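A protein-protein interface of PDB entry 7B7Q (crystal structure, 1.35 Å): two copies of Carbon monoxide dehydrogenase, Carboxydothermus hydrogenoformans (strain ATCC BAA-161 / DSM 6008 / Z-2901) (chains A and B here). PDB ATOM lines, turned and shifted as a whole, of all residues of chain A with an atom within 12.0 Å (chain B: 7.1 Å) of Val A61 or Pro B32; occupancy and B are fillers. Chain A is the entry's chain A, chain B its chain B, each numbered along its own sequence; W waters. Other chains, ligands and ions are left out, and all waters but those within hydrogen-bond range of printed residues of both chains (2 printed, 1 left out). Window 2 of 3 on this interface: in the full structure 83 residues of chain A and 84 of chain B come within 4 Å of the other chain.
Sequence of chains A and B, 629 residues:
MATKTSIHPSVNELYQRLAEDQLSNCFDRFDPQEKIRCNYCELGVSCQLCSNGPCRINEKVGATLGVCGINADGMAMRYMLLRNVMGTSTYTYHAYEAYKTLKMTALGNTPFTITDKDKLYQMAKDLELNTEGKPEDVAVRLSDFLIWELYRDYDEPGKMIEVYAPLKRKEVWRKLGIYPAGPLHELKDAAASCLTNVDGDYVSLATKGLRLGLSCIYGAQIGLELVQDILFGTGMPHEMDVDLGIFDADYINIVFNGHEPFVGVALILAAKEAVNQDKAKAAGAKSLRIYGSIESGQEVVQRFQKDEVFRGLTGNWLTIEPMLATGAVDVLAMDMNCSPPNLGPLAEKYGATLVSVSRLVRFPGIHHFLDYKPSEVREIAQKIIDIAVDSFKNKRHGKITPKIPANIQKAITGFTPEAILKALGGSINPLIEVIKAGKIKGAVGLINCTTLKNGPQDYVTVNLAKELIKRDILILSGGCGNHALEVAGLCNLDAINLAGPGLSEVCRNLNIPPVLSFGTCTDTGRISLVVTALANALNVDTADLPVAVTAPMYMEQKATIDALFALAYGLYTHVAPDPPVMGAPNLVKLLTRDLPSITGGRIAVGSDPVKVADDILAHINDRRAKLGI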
ATOM      1  N   TYR A  40      19.294  -3.599   5.354  1.00  0.00           N
ATOM      2  CA  TYR A  40      18.477  -2.737   4.494  1.00  0.00           C
ATOM      3  C   TYR A  40      17.134  -2.444   5.154  1.00  0.00           C
ATOM      4  O   TYR A  40      16.698  -1.291   5.231  1.00  0.00           O
ATOM      5  CB  TYR A  40      18.241  -3.364   3.119  1.00  0.00           C
ATOM      6  CG  TYR A  40      19.466  -3.573   2.239  1.00  0.00           C
ATOM      7  CD1 TYR A  40      19.911  -2.575   1.381  1.00  0.00           C
ATOM      8  CD2 TYR A  40      20.111  -4.817   2.184  1.00  0.00           C
ATOM      9  CE1 TYR A  40      21.012  -2.780   0.545  1.00  0.00           C
ATOM     10  CE2 TYR A  40      21.197  -5.034   1.350  1.00  0.00           C
ATOM     11  CZ  TYR A  40      21.626  -4.019   0.519  1.00  0.00           C
ATOM     12  OH  TYR A  40      22.692  -4.244  -0.331  1.00  0.00           O
ATOM     13  N   VAL A  45      15.404   1.049   3.879  1.00  0.00           N
ATOM     14  CA  VAL A  45      15.747   1.193   2.459  1.00  0.00           C
ATOM     15  C   VAL A  45      15.631  -0.116   1.682  1.00  0.00           C
ATOM     16  O   VAL A  45      16.425  -0.405   0.769  1.00  0.00           O
ATOM     17  CB  VAL A  45      17.107   1.887   2.281  1.00  0.00           C
ATOM     18  CG1 VAL A  45      17.032   3.291   2.883  1.00  0.00           C
ATOM     19  CG2 VAL A  45      18.274   1.073   2.914  1.00  0.00           C
ATOM     20  N   ASN A  52       8.077  -5.508  -9.729  1.00  0.00           N
ATOM     21  CA  ASN A  52       9.428  -5.170 -10.191  1.00  0.00           C
ATOM     22  C   ASN A  52      10.456  -5.278  -9.074  1.00  0.00           C
ATOM     23  O   ASN A  52      11.651  -5.292  -9.363  1.00  0.00           O
ATOM     24  CB  ASN A  52       9.476  -3.762 -10.816  1.00  0.00           C
ATOM     25  CG  ASN A  52       9.172  -3.740 -12.309  1.00  0.00           C
ATOM     26  OD1 ASN A  52       9.551  -4.646 -13.040  1.00  0.00           O
ATOM     27  ND2 ASN A  52       8.522  -2.661 -12.778  1.00  0.00           N
ATOM     28  N   GLY A  53      10.015  -5.303  -7.817  1.00  0.00           N
ATOM     29  CA  GLY A  53      10.870  -5.536  -6.680  1.00  0.00           C
ATOM     30  C   GLY A  53      11.119  -7.017  -6.468  1.00  0.00           C
ATOM     31  O   GLY A  53      10.933  -7.844  -7.363  1.00  0.00           O
ATOM     32  N   PRO A  54      11.558  -7.379  -5.257  1.00  0.00           N
ATOM     33  CA  PRO A  54      11.847  -6.467  -4.144  1.00  0.00           C
ATOM     34  C   PRO A  54      13.070  -5.594  -4.433  1.00  0.00           C
ATOM     35  O   PRO A  54      14.004  -6.028  -5.103  1.00  0.00           O
ATOM     36  CB  PRO A  54      12.102  -7.427  -2.982  1.00  0.00           C
ATOM     37  CG  PRO A  54      12.662  -8.645  -3.633  1.00  0.00           C
ATOM     38  CD  PRO A  54      11.934  -8.766  -4.948  1.00  0.00           C
ATOM     39  N   CYS A  55      13.027  -4.339  -3.989  1.00  0.00           N
ATOM     40  CA  CYS A  55      14.113  -3.409  -4.257  1.00  0.00           C
ATOM     41  C   CYS A  55      14.861  -3.057  -2.971  1.00  0.00           C
ATOM     42  O   CYS A  55      14.324  -3.178  -1.858  1.00  0.00           O
ATOM     43  CB  CYS A  55      13.585  -2.105  -4.872  1.00  0.00           C
ATOM     44  SG  CYS A  55      12.879  -2.337  -6.550  1.00  0.00           S
ATOM     45  N   ARG A  56      16.104  -2.585  -3.153  1.00  0.00           N
ATOM     46  CA  ARG A  56      16.981  -2.134  -2.094  1.00  0.00           C
ATOM     47  C   ARG A  56      17.782  -0.948  -2.595  1.00  0.00           C
ATOM     48  O   ARG A  56      18.104  -0.885  -3.774  1.00  0.00           O
ATOM     49  CB  ARG A  56      18.036  -3.206  -1.758  1.00  0.00           C
ATOM     50  CG  ARG A  56      17.479  -4.378  -1.037  1.00  0.00           C
ATOM     51  CD  ARG A  56      18.396  -5.595  -1.115  1.00  0.00           C
ATOM     52  NE  ARG A  56      18.179  -6.482  -0.007  1.00  0.00           N
ATOM     53  CZ  ARG A  56      18.919  -7.555   0.252  1.00  0.00           C
ATOM     54  NH1 ARG A  56      19.909  -7.942  -0.562  1.00  0.00           N
ATOM     55  NH2 ARG A  56      18.676  -8.243   1.342  1.00  0.00           N
ATOM     56  N   ILE A  57      18.158  -0.042  -1.701  1.00  0.00           N
ATOM     57  CA  ILE A  57      19.031   1.076  -2.065  1.00  0.00           C
ATOM     58  C   ILE A  57      20.477   0.687  -1.752  1.00  0.00           C
ATOM     59  O   ILE A  57      20.829   0.399  -0.598  1.00  0.00           O
ATOM     60  CB  ILE A  57      18.644   2.377  -1.337  1.00  0.00           C
ATOM     61  CG1 ILE A  57      17.177   2.770  -1.600  1.00  0.00           C
ATOM     62  CG2 ILE A  57      19.574   3.505  -1.755  1.00  0.00           C
ATOM     63  CD1 ILE A  57      16.807   2.936  -3.091  1.00  0.00           C
ATOM     64  N   ASN A  58      21.320   0.661  -2.787  1.00  0.00           N
ATOM     65  CA  ASN A  58      22.751   0.406  -2.612  1.00  0.00           C
ATOM     66  C   ASN A  58      23.455   1.213  -3.693  1.00  0.00           C
ATOM     67  O   ASN A  58      23.517   0.792  -4.854  1.00  0.00           O
ATOM     68  CB  ASN A  58      23.072  -1.084  -2.712  1.00  0.00           C
ATOM     69  CG  ASN A  58      24.553  -1.375  -2.515  1.00  0.00           C
ATOM     70  OD1 ASN A  58      25.403  -0.489  -2.638  1.00  0.00           O
ATOM     71  ND2 ASN A  58      24.876  -2.630  -2.231  1.00  0.00           N
ATOM     72  N   GLU A  59      24.012   2.354  -3.299  1.00  0.00           N
ATOM     73  CA  GLU A  59      24.628   3.229  -4.292  1.00  0.00           C
ATOM     74  C   GLU A  59      25.880   2.615  -4.929  1.00  0.00           C
ATOM     75  O   GLU A  59      26.200   2.940  -6.082  1.00  0.00           O
ATOM     76  CB  GLU A  59      24.896   4.606  -3.684  1.00  0.00           C
ATOM     77  CG  GLU A  59      23.821   5.617  -4.096  1.00  0.00           C
ATOM     78  CD  GLU A  59      23.632   6.759  -3.109  1.00  0.00           C
ATOM     79  OE1 GLU A  59      24.589   7.536  -2.906  1.00  0.00           O
ATOM     80  OE2 GLU A  59      22.520   6.876  -2.542  1.00  0.00           O
ATOM     81  N   LYS A  60      26.566   1.696  -4.238  1.00  0.00           N
ATOM     82  CA  LYS A  60      27.823   1.153  -4.764  1.00  0.00           C
ATOM     83  C   LYS A  60      27.639   0.429  -6.092  1.00  0.00           C
ATOM     84  O   LYS A  60      28.550   0.427  -6.928  1.00  0.00           O
ATOM     85  CB  LYS A  60      28.445   0.185  -3.752  1.00  0.00           C
ATOM     86  CG  LYS A  60      29.180   0.860  -2.607  1.00  0.00           C
ATOM     87  CD  LYS A  60      30.604   0.309  -2.462  1.00  0.00           C
ATOM     88  CE  LYS A  60      31.564   1.347  -1.881  1.00  0.00           C
ATOM     89  NZ  LYS A  60      32.963   0.809  -1.725  1.00  0.00           N
ATOM     90  N   VAL A  61      26.499  -0.223  -6.295  1.00  0.00           N
ATOM     91  CA  VAL A  61      26.227  -0.923  -7.539  1.00  0.00           C
ATOM     92  C   VAL A  61      25.266  -0.144  -8.426  1.00  0.00           C
ATOM     93  O   VAL A  61      24.705  -0.705  -9.358  1.00  0.00           O
ATOM     94  CB  VAL A  61      25.736  -2.355  -7.313  1.00  0.00           C
ATOM     95  CG1 VAL A  61      26.837  -3.185  -6.719  1.00  0.00           C
ATOM     96  CG2 VAL A  61      24.479  -2.361  -6.444  1.00  0.00           C
ATOM     97  N   GLY A  62      25.041   1.135  -8.128  1.00  0.00           N
ATOM     98  CA  GLY A  62      24.160   1.953  -8.925  1.00  0.00           C
ATOM     99  C   GLY A  62      22.686   1.802  -8.633  1.00  0.00           C
ATOM    100  O   GLY A  62      21.867   2.290  -9.423  1.00  0.00           O
ATOM    101  N   ALA A  63      22.326   1.109  -7.550  1.00  0.00           N
ATOM    102  CA  ALA A  63      20.929   0.962  -7.112  1.00  0.00           C
ATOM    103  C   ALA A  63      20.511   2.141  -6.225  1.00  0.00           C
ATOM    104  O   ALA A  63      20.193   2.011  -5.046  1.00  0.00           O
ATOM    105  CB  ALA A  63      20.751  -0.376  -6.402  1.00  0.00           C
ATOM    106  N   THR A  64      20.554   3.328  -6.826  1.00  0.00           N
ATOM    107  CA  THR A  64      20.240   4.568  -6.131  1.00  0.00           C
ATOM    108  C   THR A  64      18.739   4.771  -5.944  1.00  0.00           C
ATOM    109  O   THR A  64      18.321   5.415  -4.961  1.00  0.00           O
ATOM    110  CB  THR A  64      20.830   5.721  -6.945  1.00  0.00           C
ATOM    111  OG1 THR A  64      22.254   5.572  -6.971  1.00  0.00           O
ATOM    112  CG2 THR A  64      20.466   7.062  -6.354  1.00  0.00           C
ATOM    113  N   LEU A  65      17.934   4.240  -6.872  1.00  0.00           N
ATOM    114  CA  LEU A  65      16.494   4.361  -6.922  1.00  0.00           C
ATOM    115  C   LEU A  65      15.900   2.968  -7.080  1.00  0.00           C
ATOM    116  O   LEU A  65      16.538   2.063  -7.615  1.00  0.00           O
ATOM    117  CB  LEU A  65      16.056   5.281  -8.092  1.00  0.00           C
ATOM    118  CG  LEU A  65      16.637   6.711  -8.130  1.00  0.00           C
ATOM    119  CD1 LEU A  65      16.166   7.417  -9.392  1.00  0.00           C
ATOM    120  CD2 LEU A  65      16.283   7.537  -6.902  1.00  0.00           C
ATOM    121  N   GLY A  66      14.643   2.806  -6.635  1.00  0.00           N
ATOM    122  CA  GLY A  66      13.880   1.617  -6.988  1.00  0.00           C
ATOM    123  C   GLY A  66      13.618   1.562  -8.482  1.00  0.00           C
ATOM    124  O   GLY A  66      13.808   2.548  -9.197  1.00  0.00           O
ATOM    125  N   VAL A  67      13.173   0.391  -8.979  1.00  0.00           N
ATOM    126  CA  VAL A  67      12.917   0.276 -10.422  1.00  0.00           C
ATOM    127  C   VAL A  67      11.979   1.384 -10.890  1.00  0.00           C
ATOM    128  O   VAL A  67      12.171   1.974 -11.968  1.00  0.00           O
ATOM    129  CB  VAL A  67      12.385  -1.127 -10.801  1.00  0.00           C
ATOM    130  CG1 VAL A  67      12.150  -1.217 -12.316  1.00  0.00           C
ATOM    131  CG2 VAL A  67      13.328  -2.213 -10.375  1.00  0.00           C
ATOM    132  N   CYS A  68      10.951   1.689 -10.098  1.00  0.00           N
ATOM    133  CA  CYS A  68       9.953   2.701 -10.454  1.00  0.00           C
ATOM    134  C   CYS A  68      10.499   4.123 -10.447  1.00  0.00           C
ATOM    135  O   CYS A  68       9.844   5.018 -10.992  1.00  0.00           O
ATOM    136  CB  CYS A  68       8.775   2.632  -9.471  1.00  0.00           C
ATOM    137  SG  CYS A  68       9.290   2.900  -7.734  1.00  0.00           S
ATOM    138  N   GLY A  69      11.649   4.359  -9.805  1.00  0.00           N
ATOM    139  CA  GLY A  69      12.266   5.670  -9.696  1.00  0.00           C
ATOM    140  C   GLY A  69      12.208   6.319  -8.312  1.00  0.00           C
ATOM    141  O   GLY A  69      12.682   7.456  -8.164  1.00  0.00           O
ATOM    142  N   ILE A  70      11.606   5.672  -7.299  1.00  0.00           N
ATOM    143  CA  ILE A  70      11.516   6.277  -5.963  1.00  0.00           C
ATOM    144  C   ILE A  70      12.891   6.293  -5.293  1.00  0.00           C
ATOM    145  O   ILE A  70      13.691   5.360  -5.445  1.00  0.00           O
ATOM    146  CB  ILE A  70      10.446   5.584  -5.094  1.00  0.00           C
ATOM    147  CG1 ILE A  70       9.979   6.487  -3.922  1.00  0.00           C
ATOM    148  CG2 ILE A  70      10.913   4.209  -4.579  1.00  0.00           C
ATOM    149  CD1 ILE A  70       8.750   5.984  -3.191  1.00  0.00           C
ATOM    150  N   MET A  75      10.900   6.005  -0.189  1.00  0.00           N
ATOM    151  CA  MET A  75      10.731   4.600   0.148  1.00  0.00           C
ATOM    152  C   MET A  75      10.469   4.430   1.647  1.00  0.00           C
ATOM    153  O   MET A  75       9.509   3.757   2.062  1.00  0.00           O
ATOM    154  CB  MET A  75      11.993   3.848  -0.271  1.00  0.00           C
ATOM    155  CG  MET A  75      11.922   2.338  -0.078  1.00  0.00           C
ATOM    156  SD  MET A  75      13.424   1.483  -0.630  1.00  0.00           S
ATOM    157  CE  MET A  75      13.308   1.688  -2.405  1.00  0.00           C
ATOM    158  N   PHE B  27      13.883   0.791 -17.355  1.00  0.00           N
ATOM    159  CA  PHE B  27      14.588  -0.327 -17.992  1.00  0.00           C
ATOM    160  C   PHE B  27      16.005  -0.468 -17.435  1.00  0.00           C
ATOM    161  O   PHE B  27      16.433  -1.568 -17.052  1.00  0.00           O
ATOM    162  CB  PHE B  27      14.613  -0.159 -19.523  1.00  0.00           C
ATOM    163  CG  PHE B  27      13.240   0.141 -20.120  1.00  0.00           C
ATOM    164  CD1 PHE B  27      12.294  -0.860 -20.301  1.00  0.00           C
ATOM    165  CD2 PHE B  27      12.893   1.455 -20.456  1.00  0.00           C
ATOM    166  CE1 PHE B  27      11.017  -0.572 -20.825  1.00  0.00           C
ATOM    167  CE2 PHE B  27      11.628   1.755 -20.966  1.00  0.00           C
ATOM    168  CZ  PHE B  27      10.688   0.729 -21.148  1.00  0.00           C
ATOM    169  N   ASP B  28      16.760   0.639 -17.380  1.00  0.00           N
ATOM    170  CA  ASP B  28      18.116   0.599 -16.836  1.00  0.00           C
ATOM    171  C   ASP B  28      18.127   0.341 -15.332  1.00  0.00           C
ATOM    172  O   ASP B  28      19.021  -0.349 -14.837  1.00  0.00           O
ATOM    173  CB  ASP B  28      18.859   1.888 -17.198  1.00  0.00           C
ATOM    174  CG  ASP B  28      19.261   1.935 -18.673  1.00  0.00           C
ATOM    175  OD1 ASP B  28      19.455   0.852 -19.276  1.00  0.00           O
ATOM    176  OD2 ASP B  28      19.372   3.048 -19.248  1.00  0.00           O
ATOM    177  N   ARG B  29      17.152   0.870 -14.583  1.00  0.00           N
ATOM    178  CA  ARG B  29      17.178   0.693 -13.127  1.00  0.00           C
ATOM    179  C   ARG B  29      16.900  -0.741 -12.694  1.00  0.00           C
ATOM    180  O   ARG B  29      17.196  -1.098 -11.551  1.00  0.00           O
ATOM    181  CB  ARG B  29      16.171   1.624 -12.431  1.00  0.00           C
ATOM    182  CG  ARG B  29      16.556   3.087 -12.442  1.00  0.00           C
ATOM    183  CD  ARG B  29      15.616   3.990 -11.609  1.00  0.00           C
ATOM    184  NE  ARG B  29      14.235   3.982 -12.079  1.00  0.00           N
ATOM    185  CZ  ARG B  29      13.683   4.928 -12.834  1.00  0.00           C
ATOM    186  NH1 ARG B  29      14.385   5.978 -13.234  1.00  0.00           N
ATOM    187  NH2 ARG B  29      12.415   4.803 -13.209  1.00  0.00           N
ATOM    188  N   PHE B  30      16.308  -1.554 -13.568  1.00  0.00           N
ATOM    189  CA  PHE B  30      16.074  -2.960 -13.243  1.00  0.00           C
ATOM    190  C   PHE B  30      17.387  -3.693 -12.986  1.00  0.00           C
ATOM    191  O   PHE B  30      17.460  -4.557 -12.100  1.00  0.00           O
ATOM    192  CB  PHE B  30      15.271  -3.607 -14.380  1.00  0.00           C
ATOM    193  CG  PHE B  30      14.700  -4.966 -14.038  1.00  0.00           C
ATOM    194  CD1 PHE B  30      13.456  -5.082 -13.417  1.00  0.00           C
ATOM    195  CD2 PHE B  30      15.399  -6.121 -14.348  1.00  0.00           C
ATOM    196  CE1 PHE B  30      12.949  -6.326 -13.093  1.00  0.00           C
ATOM    197  CE2 PHE B  30      14.875  -7.362 -14.044  1.00  0.00           C
ATOM    198  CZ  PHE B  30      13.640  -7.457 -13.415  1.00  0.00           C
ATOM    199  N   ASP B  31      18.450  -3.345 -13.749  1.00  0.00           N
ATOM    200  CA  ASP B  31      19.686  -4.130 -13.712  1.00  0.00           C
ATOM    201  C   ASP B  31      20.390  -4.046 -12.359  1.00  0.00           C
ATOM    202  O   ASP B  31      20.791  -5.095 -11.822  1.00  0.00           O
ATOM    203  CB  ASP B  31      20.603  -3.718 -14.875  1.00  0.00           C
ATOM    204  CG  ASP B  31      20.054  -4.107 -16.240  1.00  0.00           C
ATOM    205  OD1 ASP B  31      19.322  -5.114 -16.338  1.00  0.00           O
ATOM    206  OD2 ASP B  31      20.383  -3.405 -17.240  1.00  0.00           O
ATOM    207  N   PRO B  32      20.605  -2.876 -11.778  1.00  0.00           N
ATOM    208  CA  PRO B  32      21.249  -2.853 -10.454  1.00  0.00           C
ATOM    209  C   PRO B  32      20.456  -3.591  -9.390  1.00  0.00           C
ATOM    210  O   PRO B  32      21.044  -4.253  -8.538  1.00  0.00           O
ATOM    211  CB  PRO B  32      21.389  -1.362 -10.152  1.00  0.00           C
ATOM    212  CG  PRO B  32      21.446  -0.726 -11.486  1.00  0.00           C
ATOM    213  CD  PRO B  32      20.500  -1.520 -12.349  1.00  0.00           C
ATOM    214  N   GLN B  33      19.122  -3.507  -9.426  1.00  0.00           N
ATOM    215  CA  GLN B  33      18.315  -4.266  -8.468  1.00  0.00           C
ATOM    216  C   GLN B  33      18.531  -5.773  -8.626  1.00  0.00           C
ATOM    217  O   GLN B  33      18.555  -6.519  -7.635  1.00  0.00           O
ATOM    218  CB  GLN B  33      16.827  -3.880  -8.596  1.00  0.00           C
ATOM    219  CG  GLN B  33      16.534  -2.429  -8.242  1.00  0.00           C
ATOM    220  CD  GLN B  33      16.824  -2.116  -6.785  1.00  0.00           C
ATOM    221  OE1 GLN B  33      16.801  -3.014  -5.933  1.00  0.00           O
ATOM    222  NE2 GLN B  33      17.025  -0.833  -6.475  1.00  0.00           N
ATOM    223  N   GLU B  34      18.708  -6.234  -9.871  1.00  0.00           N
ATOM    224  CA  GLU B  34      18.956  -7.652 -10.150  1.00  0.00           C
ATOM    225  C   GLU B  34      20.226  -8.159  -9.500  1.00  0.00           C
ATOM    226  O   GLU B  34      20.341  -9.359  -9.214  1.00  0.00           O
ATOM    227  CB  GLU B  34      19.097  -7.859 -11.656  1.00  0.00           C
ATOM    228  CG  GLU B  34      17.790  -7.840 -12.339  1.00  0.00           C
ATOM    229  CD  GLU B  34      17.009  -9.069 -12.028  1.00  0.00           C
ATOM    230  OE1 GLU B  34      17.207 -10.081 -12.747  1.00  0.00           O
ATOM    231  OE2 GLU B  34      16.216  -9.013 -11.057  1.00  0.00           O
ATOM    232  N   LYS B  35      21.202  -7.292  -9.293  1.00  0.00           N
ATOM    233  CA  LYS B  35      22.451  -7.736  -8.688  1.00  0.00           C
ATOM    234  C   LYS B  35      22.267  -8.115  -7.228  1.00  0.00           C
ATOM    235  O   LYS B  35      23.035  -8.925  -6.697  1.00  0.00           O
ATOM    236  CB  LYS B  35      23.511  -6.636  -8.770  1.00  0.00           C
ATOM    237  CG  LYS B  35      24.174  -6.487 -10.118  1.00  0.00           C
ATOM    238  CD  LYS B  35      25.313  -5.486 -10.071  1.00  0.00           C
ATOM    239  CE  LYS B  35      26.130  -5.518 -11.364  1.00  0.00           C
ATOM    240  NZ  LYS B  35      26.752  -6.862 -11.616  1.00  0.00           N
ATOM    241  N   ILE B  36      21.279  -7.534  -6.549  1.00  0.00           N
ATOM    242  CA  ILE B  36      21.210  -7.622  -5.092  1.00  0.00           C
ATOM    243  C   ILE B  36      19.846  -8.094  -4.591  1.00  0.00           C
ATOM    244  O   ILE B  36      19.471  -7.816  -3.449  1.00  0.00           O
ATOM    245  CB  ILE B  36      21.637  -6.289  -4.443  1.00  0.00           C
ATOM    246  CG1 ILE B  36      20.717  -5.133  -4.857  1.00  0.00           C
ATOM    247  CG2 ILE B  36      23.102  -6.000  -4.738  1.00  0.00           C
ATOM    248  CD1 ILE B  36      21.045  -3.786  -4.176  1.00  0.00           C
ATOM    249  N   ARG B  37      19.111  -8.857  -5.400  1.00  0.00           N
ATOM    250  CA  ARG B  37      17.764  -9.277  -5.010  1.00  0.00           C
ATOM    251  C   ARG B  37      17.768 -10.090  -3.724  1.00  0.00           C
ATOM    252  O   ARG B  37      18.511 -11.066  -3.595  1.00  0.00           O
ATOM    253  CB  ARG B  37      17.126 -10.126  -6.116  1.00  0.00           C
ATOM    254  CG  ARG B  37      16.878  -9.419  -7.401  1.00  0.00           C
ATOM    255  CD  ARG B  37      15.826  -8.337  -7.268  1.00  0.00           C
ATOM    256  NE  ARG B  37      15.438  -7.869  -8.594  1.00  0.00           N
ATOM    257  CZ  ARG B  37      14.528  -6.914  -8.846  1.00  0.00           C
ATOM    258  NH1 ARG B  37      14.243  -6.585 -10.101  1.00  0.00           N
ATOM    259  NH2 ARG B  37      13.914  -6.266  -7.866  1.00  0.00           N
HETATM  260  O   HOH W   1      10.297   7.272 -12.651  1.00  0.00           O
HETATM  261  O   HOH W   2      18.125   0.750  -9.522  1.00  0.00           O
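The backbone carbonyl oxygen of Leu A65 lies within hydrogen-bond range of the side-chain amide nitrogen of Gln B33 (3.2 Å).
The backbone carbonyl oxygen of Asn A52 is in hydrogen-bond range of the guanidinium group of Arg B37, at 2.9 Å.
NH1 of Arg A56 lies within hydrogen-bond range of O of Ile B36, 2.9 Å away.
NE of Arg B29 sits at hydrogen-bond distance from O of Gly A66 (3.2 Å).
NH2 of Arg B37 sits at hydrogen-bond distance from O of Pro A54, 2.8 Å away.
The guanidinium group of Arg B29 sits at hydrogen-bond distance from the backbone carbonyl oxygen of Cys A68 (3.4 Å).
The backbone carbonyl oxygen (O) of Val A67 lies within hydrogen-bond range of the guanidinium group (NE) of Arg B29, 2.9 Å away.
N of Arg A56 lies within hydrogen-bond range of OE1 of Gln B33, 2.9 Å away.
The guanidinium group of Arg B29 lies close to the backbone NH of Gly A69.
O of Gly A53 lies close to NH2 of Arg B37, 3.4 Å away.
The side-chain carboxylate of Glu B34 lies within salt-bridge range of the guanidinium group of Arg B37 (2.8 Å).
SG of Cys A55 lies close to N of Val A67 (3.7 Å).
OD1 of Asn A58 lies within hydrogen-bond range of N of Lys A60, 2.9 Å away.
The backbone NH (N) of Asn A58 lies within hydrogen-bond range of the backbone carbonyl oxygen (O) of Ala A63, at 2.9 Å.
The side-chain sulfur (SG) of Cys A68 lies close to the backbone NH (N) of Ile A70 (3.6 Å).
The side-chain hydroxyl (OH) of Tyr A40 is in hydrogen-bond range of the side-chain amide nitrogen (ND2) of Asn A58.
Among the printed residues, merely in contact across the chains: Asn A52 with Phe B30 (3.8 Å), Cys A55 with Gln B33 (3.2 Å), Asn A58 with Ile B36 (3.7 Å), Val A61 with Pro B32 (3.5 Å), Gly A62 with Pro B32 (3.7 Å), Ala A63 with Pro B32 (3.7 Å), Ala A63 with Gln B33 (3.8 Å), Leu A65 with Arg B29 (3.8 Å) and Val A67 with Gln B33 (3.9 Å).
Printed residues of chain B within 4 Å of Val A61: Pro B32 (3.5 Å).
Pro B32 touches three residues of chain A.
No residue of chain A comes within 4 Å of Asp B31.
Printed residues of chain B within 4 Å of Gly A69: Arg B29 (3.5 Å).
Printed residues of chain B within 4 Å of Gly A66: Arg B29.
Ile A70 touches none of the printed residues of chain B.
Tyr A40 touches none of the printed residues of chain B.
The nearest residue of chain B that does not touch Val A61 is Lys B35 (4.2 Å).
The nearest printed residue of chain B that does not touch Asn A52 is Gln B33 (5.4 Å).
Among the printed residues, no Asp or Glu carboxylate lies within 4 Å of a Lys or Arg side-chain nitrogen of the other chain.
No position is printed for both chains.
Water W2 lies within hydrogen-bond range of O of Leu A65 (2.8 Å) and O of Arg B29 (2.9 Å).
Water W1 bridges the backbone carbonyl oxygen (O) of Cys A68 and the guanidinium group (NH2) of Arg B29.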
